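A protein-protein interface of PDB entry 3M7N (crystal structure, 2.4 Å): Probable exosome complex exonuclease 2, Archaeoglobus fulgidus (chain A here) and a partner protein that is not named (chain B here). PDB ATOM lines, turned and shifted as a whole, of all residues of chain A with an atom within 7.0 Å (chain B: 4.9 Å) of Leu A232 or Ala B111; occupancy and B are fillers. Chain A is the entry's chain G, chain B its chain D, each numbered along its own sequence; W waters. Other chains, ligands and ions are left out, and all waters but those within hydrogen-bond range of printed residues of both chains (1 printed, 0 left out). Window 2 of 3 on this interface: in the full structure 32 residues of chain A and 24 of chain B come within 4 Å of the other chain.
Of the printed residues of chain B, Lys A227 touches Ile B201 (3.3 Å) and Ala B202 (3.0 Å). Of the printed residues of chain B, Gly A229 touches Glu B107. Leu A232 touches four residues of chain B. Of the printed residues of chain B, Leu A233 touches Ser B200 (3.5 Å) and Ile B201 (2.8 Å). Leu A237 touches none of the printed residues of chain B. Lys B156 touches none of the printed residues of chain A. Of the printed residues of chain A, Ser B200 touches Leu A232 (3.6 Å) and Leu A233 (3.5 Å).
The side-chain carboxylate of Glu B107 lies within hydrogen-bond range of the backbone NH of Gly A229, 2.7 Å away. The backbone carbonyl oxygen (O) of Leu A233 lies within hydrogen-bond range of the backbone NH (N) of Ile B201 (2.8 Å). The backbone carbonyl oxygen of Ala B202 sits at hydrogen-bond distance from the side-chain amino group of Lys A227, 3.0 Å away.
Ile B201 touches Lys A227. Glu B107 touches Gly A230 (O to CA, 3.5 Å). Tyr A231 touches Ala B111. CD1 of Leu A232 touches O of Ala B111, at 3.4 Å. Leu A232 touches Leu B192. Ser B200 touches Leu A232 (OG to CB, 3.6 Å). CA of Leu A232 touches O of Ile B201 (3.7 Å). Ser B200 touches Leu A233.
Water W1 lies within hydrogen-bond range of O of Gly A229 (2.5 Å), NZ of Lys A227 (3.0 Å) and OE1 of Glu B107 (3.5 Å).
The backbone carbonyl oxygen of Tyr A231 lies within hydrogen-bond range of the side-chain amino group of Lys A227, 2.7 Å away. The backbone carbonyl oxygen (O) of Ser B200 lies within hydrogen-bond range of the backbone NH (N) of Leu B192.
Of the 11 printed residues of chain A, 6 touch a printed residue of chain B. Hydrophobic or aromatic side chains of chain B that line the printed part of chain A: Ala B111, Leu B192 and Ile B201. Among the printed residues, 11 pairs touch across the chains. Among the printed residues, no Asp or Glu carboxylate lies within 4 Å of a Lys or Arg side-chain nitrogen of the other chain.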
ATOM      1  N   ILE A 191     -22.680  30.822  13.108  1.00  0.00           N
ATOM      2  CA  ILE A 191     -22.814  29.366  13.057  1.00  0.00           C
ATOM      3  C   ILE A 191     -21.592  28.714  12.414  1.00  0.00           C
ATOM      4  O   ILE A 191     -21.191  29.066  11.318  1.00  0.00           O
ATOM      5  CB  ILE A 191     -24.133  28.885  12.374  1.00  0.00           C
ATOM      6  CG1 ILE A 191     -25.357  29.258  13.217  1.00  0.00           C
ATOM      7  CG2 ILE A 191     -24.143  27.356  12.212  1.00  0.00           C
ATOM      8  CD1 ILE A 191     -25.909  30.604  12.925  1.00  0.00           C
ATOM      9  N   GLY A 193     -20.578  24.953  11.692  1.00  0.00           N
ATOM     10  CA  GLY A 193     -20.984  23.561  11.738  1.00  0.00           C
ATOM     11  C   GLY A 193     -22.222  23.451  12.607  1.00  0.00           C
ATOM     12  O   GLY A 193     -23.220  24.127  12.363  1.00  0.00           O
ATOM     13  N   THR A 210     -20.956  33.350   8.325  1.00  0.00           N
ATOM     14  CA  THR A 210     -22.114  32.463   8.411  1.00  0.00           C
ATOM     15  C   THR A 210     -22.882  32.660   9.706  1.00  0.00           C
ATOM     16  O   THR A 210     -22.499  32.141  10.748  1.00  0.00           O
ATOM     17  CB  THR A 210     -21.665  31.029   8.350  1.00  0.00           C
ATOM     18  OG1 THR A 210     -20.629  30.842   9.316  1.00  0.00           O
ATOM     19  CG2 THR A 210     -21.105  30.712   6.960  1.00  0.00           C
ATOM     20  N   LYS A 227     -31.240  34.437   8.200  1.00  0.00           N
ATOM     21  CA  LYS A 227     -30.055  33.614   8.042  1.00  0.00           C
ATOM     22  C   LYS A 227     -29.185  34.242   6.937  1.00  0.00           C
ATOM     23  O   LYS A 227     -29.727  34.735   5.944  1.00  0.00           O
ATOM     24  CB  LYS A 227     -30.475  32.192   7.654  1.00  0.00           C
ATOM     25  CG  LYS A 227     -29.315  31.272   7.291  1.00  0.00           C
ATOM     26  CD  LYS A 227     -29.804  29.912   6.761  1.00  0.00           C
ATOM     27  CE  LYS A 227     -28.638  29.036   6.296  1.00  0.00           C
ATOM     28  NZ  LYS A 227     -28.099  29.468   4.981  1.00  0.00           N
ATOM     29  N   GLY A 229     -25.158  34.158   4.715  1.00  0.00           N
ATOM     30  CA  GLY A 229     -23.904  33.492   4.428  1.00  0.00           C
ATOM     31  C   GLY A 229     -24.103  32.157   3.746  1.00  0.00           C
ATOM     32  O   GLY A 229     -25.218  31.640   3.713  1.00  0.00           O
ATOM     33  N   GLY A 230     -23.019  31.593   3.218  1.00  0.00           N
ATOM     34  CA  GLY A 230     -23.085  30.364   2.447  1.00  0.00           C
ATOM     35  C   GLY A 230     -22.902  29.100   3.263  1.00  0.00           C
ATOM     36  O   GLY A 230     -21.866  28.433   3.182  1.00  0.00           O
ATOM     37  N   TYR A 231     -23.914  28.752   4.051  1.00  0.00           N
ATOM     38  CA  TYR A 231     -23.815  27.559   4.883  1.00  0.00           C
ATOM     39  C   TYR A 231     -25.190  26.925   5.047  1.00  0.00           C
ATOM     40  O   TYR A 231     -26.219  27.591   4.858  1.00  0.00           O
ATOM     41  CB  TYR A 231     -23.221  27.918   6.258  1.00  0.00           C
ATOM     42  CG  TYR A 231     -24.211  28.569   7.199  1.00  0.00           C
ATOM     43  CD1 TYR A 231     -24.784  27.849   8.247  1.00  0.00           C
ATOM     44  CD2 TYR A 231     -24.591  29.906   7.034  1.00  0.00           C
ATOM     45  CE1 TYR A 231     -25.708  28.447   9.120  1.00  0.00           C
ATOM     46  CE2 TYR A 231     -25.513  30.510   7.893  1.00  0.00           C
ATOM     47  CZ  TYR A 231     -26.064  29.774   8.937  1.00  0.00           C
ATOM     48  OH  TYR A 231     -26.988  30.359   9.792  1.00  0.00           O
ATOM     49  N   LEU A 232     -25.208  25.643   5.405  1.00  0.00           N
ATOM     50  CA  LEU A 232     -26.460  24.952   5.708  1.00  0.00           C
ATOM     51  C   LEU A 232     -26.757  24.986   7.214  1.00  0.00           C
ATOM     52  O   LEU A 232     -25.924  24.595   8.022  1.00  0.00           O
ATOM     53  CB  LEU A 232     -26.397  23.512   5.194  1.00  0.00           C
ATOM     54  CG  LEU A 232     -26.252  23.449   3.666  1.00  0.00           C
ATOM     55  CD1 LEU A 232     -25.585  22.163   3.205  1.00  0.00           C
ATOM     56  CD2 LEU A 232     -27.608  23.656   2.992  1.00  0.00           C
ATOM     57  N   LEU A 233     -27.937  25.479   7.574  1.00  0.00           N
ATOM     58  CA  LEU A 233     -28.358  25.570   8.960  1.00  0.00           C
ATOM     59  C   LEU A 233     -29.086  24.284   9.369  1.00  0.00           C
ATOM     60  O   LEU A 233     -30.087  23.904   8.756  1.00  0.00           O
ATOM     61  CB  LEU A 233     -29.306  26.749   9.127  1.00  0.00           C
ATOM     62  CG  LEU A 233     -29.352  27.471  10.473  1.00  0.00           C
ATOM     63  CD1 LEU A 233     -30.781  27.864  10.850  1.00  0.00           C
ATOM     64  CD2 LEU A 233     -28.701  26.648  11.569  1.00  0.00           C
ATOM     65  N   ASP A 234     -28.581  23.616  10.403  1.00  0.00           N
ATOM     66  CA  ASP A 234     -29.228  22.422  10.931  1.00  0.00           C
ATOM     67  C   ASP A 234     -30.477  22.813  11.722  1.00  0.00           C
ATOM     68  O   ASP A 234     -30.460  23.774  12.487  1.00  0.00           O
ATOM     69  CB  ASP A 234     -28.252  21.630  11.803  1.00  0.00           C
ATOM     70  CG  ASP A 234     -28.935  20.535  12.598  1.00  0.00           C
ATOM     71  OD1 ASP A 234     -29.586  20.848  13.623  1.00  0.00           O
ATOM     72  OD2 ASP A 234     -28.807  19.360  12.201  1.00  0.00           O
ATOM     73  N   LEU A 237     -30.276  22.664  15.747  1.00  0.00           N
ATOM     74  CA  LEU A 237     -29.540  23.838  16.185  1.00  0.00           C
ATOM     75  C   LEU A 237     -30.477  25.021  16.169  1.00  0.00           C
ATOM     76  O   LEU A 237     -30.569  25.774  17.140  1.00  0.00           O
ATOM     77  CB  LEU A 237     -28.371  24.098  15.245  1.00  0.00           C
ATOM     78  CG  LEU A 237     -27.135  24.726  15.872  1.00  0.00           C
ATOM     79  CD1 LEU A 237     -26.117  25.098  14.805  1.00  0.00           C
ATOM     80  CD2 LEU A 237     -27.549  25.938  16.647  1.00  0.00           C
ATOM     81  N   GLU B 107     -26.432  33.022  -1.546  1.00  0.00           N
ATOM     82  CA  GLU B 107     -25.883  32.337  -0.374  1.00  0.00           C
ATOM     83  C   GLU B 107     -26.409  30.901  -0.267  1.00  0.00           C
ATOM     84  O   GLU B 107     -25.691  29.989   0.127  1.00  0.00           O
ATOM     85  CB  GLU B 107     -26.147  33.135   0.908  1.00  0.00           C
ATOM     86  CG  GLU B 107     -25.130  34.226   1.104  1.00  0.00           C
ATOM     87  CD  GLU B 107     -25.596  35.359   1.991  1.00  0.00           C
ATOM     88  OE1 GLU B 107     -26.627  35.239   2.692  1.00  0.00           O
ATOM     89  OE2 GLU B 107     -24.903  36.392   1.980  1.00  0.00           O
ATOM     90  N   ALA B 108     -27.659  30.711  -0.653  1.00  0.00           N
ATOM     91  CA  ALA B 108     -28.287  29.396  -0.596  1.00  0.00           C
ATOM     92  C   ALA B 108     -27.630  28.424  -1.553  1.00  0.00           C
ATOM     93  O   ALA B 108     -27.529  27.238  -1.254  1.00  0.00           O
ATOM     94  CB  ALA B 108     -29.786  29.498  -0.872  1.00  0.00           C
ATOM     95  N   PHE B 109     -27.171  28.905  -2.701  1.00  0.00           N
ATOM     96  CA  PHE B 109     -26.545  27.983  -3.657  1.00  0.00           C
ATOM     97  C   PHE B 109     -25.059  27.754  -3.401  1.00  0.00           C
ATOM     98  O   PHE B 109     -24.498  26.738  -3.831  1.00  0.00           O
ATOM     99  CB  PHE B 109     -26.809  28.402  -5.107  1.00  0.00           C
ATOM    100  CG  PHE B 109     -28.222  28.198  -5.533  1.00  0.00           C
ATOM    101  CD1 PHE B 109     -29.076  29.267  -5.668  1.00  0.00           C
ATOM    102  CD2 PHE B 109     -28.708  26.925  -5.768  1.00  0.00           C
ATOM    103  CE1 PHE B 109     -30.392  29.072  -6.042  1.00  0.00           C
ATOM    104  CE2 PHE B 109     -30.013  26.727  -6.148  1.00  0.00           C
ATOM    105  CZ  PHE B 109     -30.858  27.795  -6.290  1.00  0.00           C
ATOM    106  N   GLU B 110     -24.427  28.695  -2.701  1.00  0.00           N
ATOM    107  CA  GLU B 110     -23.025  28.545  -2.295  1.00  0.00           C
ATOM    108  C   GLU B 110     -22.878  27.355  -1.352  1.00  0.00           C
ATOM    109  O   GLU B 110     -21.849  26.681  -1.322  1.00  0.00           O
ATOM    110  CB  GLU B 110     -22.523  29.830  -1.618  1.00  0.00           C
ATOM    111  CG  GLU B 110     -21.947  30.848  -2.593  1.00  0.00           C
ATOM    112  CD  GLU B 110     -21.744  32.214  -1.969  1.00  0.00           C
ATOM    113  OE1 GLU B 110     -22.407  32.525  -0.948  1.00  0.00           O
ATOM    114  OE2 GLU B 110     -20.925  32.986  -2.512  1.00  0.00           O
ATOM    115  N   ALA B 111     -23.941  27.096  -0.598  1.00  0.00           N
ATOM    116  CA  ALA B 111     -23.975  26.021   0.387  1.00  0.00           C
ATOM    117  C   ALA B 111     -24.171  24.636  -0.246  1.00  0.00           C
ATOM    118  O   ALA B 111     -24.284  23.642   0.470  1.00  0.00           O
ATOM    119  CB  ALA B 111     -25.094  26.304   1.400  1.00  0.00           C
ATOM    120  N   VAL B 112     -24.187  24.574  -1.579  1.00  0.00           N
ATOM    121  CA  VAL B 112     -24.717  23.418  -2.300  1.00  0.00           C
ATOM    122  C   VAL B 112     -23.961  23.083  -3.594  1.00  0.00           C
ATOM    123  O   VAL B 112     -23.518  21.950  -3.791  1.00  0.00           O
ATOM    124  CB  VAL B 112     -26.216  23.632  -2.596  1.00  0.00           C
ATOM    125  CG1 VAL B 112     -26.627  22.894  -3.834  1.00  0.00           C
ATOM    126  CG2 VAL B 112     -27.061  23.220  -1.387  1.00  0.00           C
ATOM    127  N   ILE B 113     -23.818  24.063  -4.480  1.00  0.00           N
ATOM    128  CA  ILE B 113     -22.978  23.895  -5.667  1.00  0.00           C
ATOM    129  C   ILE B 113     -21.562  23.466  -5.271  1.00  0.00           C
ATOM    130  O   ILE B 113     -20.970  24.042  -4.365  1.00  0.00           O
ATOM    131  CB  ILE B 113     -22.913  25.199  -6.476  1.00  0.00           C
ATOM    132  CG1 ILE B 113     -24.265  25.463  -7.134  1.00  0.00           C
ATOM    133  CG2 ILE B 113     -21.826  25.128  -7.524  1.00  0.00           C
ATOM    134  CD1 ILE B 113     -24.396  26.866  -7.724  1.00  0.00           C
ATOM    135  N   LYS B 156     -24.694  19.250  -4.120  1.00  0.00           N
ATOM    136  CA  LYS B 156     -24.947  18.319  -3.037  1.00  0.00           C
ATOM    137  C   LYS B 156     -26.356  17.706  -3.111  1.00  0.00           C
ATOM    138  O   LYS B 156     -26.585  16.605  -2.616  1.00  0.00           O
ATOM    139  CB  LYS B 156     -24.753  19.023  -1.692  1.00  0.00           C
ATOM    140  CG  LYS B 156     -23.303  19.210  -1.288  1.00  0.00           C
ATOM    141  CD  LYS B 156     -23.209  20.123  -0.070  1.00  0.00           C
ATOM    142  CE  LYS B 156     -21.822  20.090   0.563  1.00  0.00           C
ATOM    143  NZ  LYS B 156     -21.752  20.966   1.774  1.00  0.00           N
ATOM    144  N   LEU B 192     -32.086  22.161   1.520  1.00  0.00           N
ATOM    145  CA  LEU B 192     -31.333  21.176   0.781  1.00  0.00           C
ATOM    146  C   LEU B 192     -32.132  19.874   0.837  1.00  0.00           C
ATOM    147  O   LEU B 192     -32.616  19.481   1.908  1.00  0.00           O
ATOM    148  CB  LEU B 192     -29.973  20.959   1.431  1.00  0.00           C
ATOM    149  CG  LEU B 192     -29.256  19.700   0.948  1.00  0.00           C
ATOM    150  CD1 LEU B 192     -28.789  19.864  -0.496  1.00  0.00           C
ATOM    151  CD2 LEU B 192     -28.091  19.337   1.850  1.00  0.00           C
ATOM    152  N   SER B 200     -31.380  20.013   5.546  1.00  0.00           N
ATOM    153  CA  SER B 200     -31.036  21.238   6.271  1.00  0.00           C
ATOM    154  C   SER B 200     -31.666  22.495   5.672  1.00  0.00           C
ATOM    155  O   SER B 200     -32.295  22.447   4.615  1.00  0.00           O
ATOM    156  CB  SER B 200     -29.520  21.406   6.337  1.00  0.00           C
ATOM    157  OG  SER B 200     -28.920  20.964   5.132  1.00  0.00           O
ATOM    158  N   ILE B 201     -31.495  23.616   6.366  1.00  0.00           N
ATOM    159  CA  ILE B 201     -32.056  24.890   5.935  1.00  0.00           C
ATOM    160  C   ILE B 201     -31.018  25.723   5.186  1.00  0.00           C
ATOM    161  O   ILE B 201     -29.978  26.069   5.748  1.00  0.00           O
ATOM    162  CB  ILE B 201     -32.564  25.695   7.135  1.00  0.00           C
ATOM    163  CG1 ILE B 201     -33.621  24.887   7.886  1.00  0.00           C
ATOM    164  CG2 ILE B 201     -33.093  27.066   6.687  1.00  0.00           C
ATOM    165  CD1 ILE B 201     -33.938  25.404   9.267  1.00  0.00           C
ATOM    166  N   ALA B 202     -31.323  26.045   3.926  1.00  0.00           N
ATOM    167  CA  ALA B 202     -30.453  26.849   3.060  1.00  0.00           C
ATOM    168  C   ALA B 202     -30.863  28.320   3.054  1.00  0.00           C
ATOM    169  O   ALA B 202     -30.058  29.200   2.752  1.00  0.00           O
ATOM    170  CB  ALA B 202     -30.475  26.298   1.644  1.00  0.00           C
HETATM  171  O   HOH W   1     -27.568  32.304   4.300  1.00  0.00           O
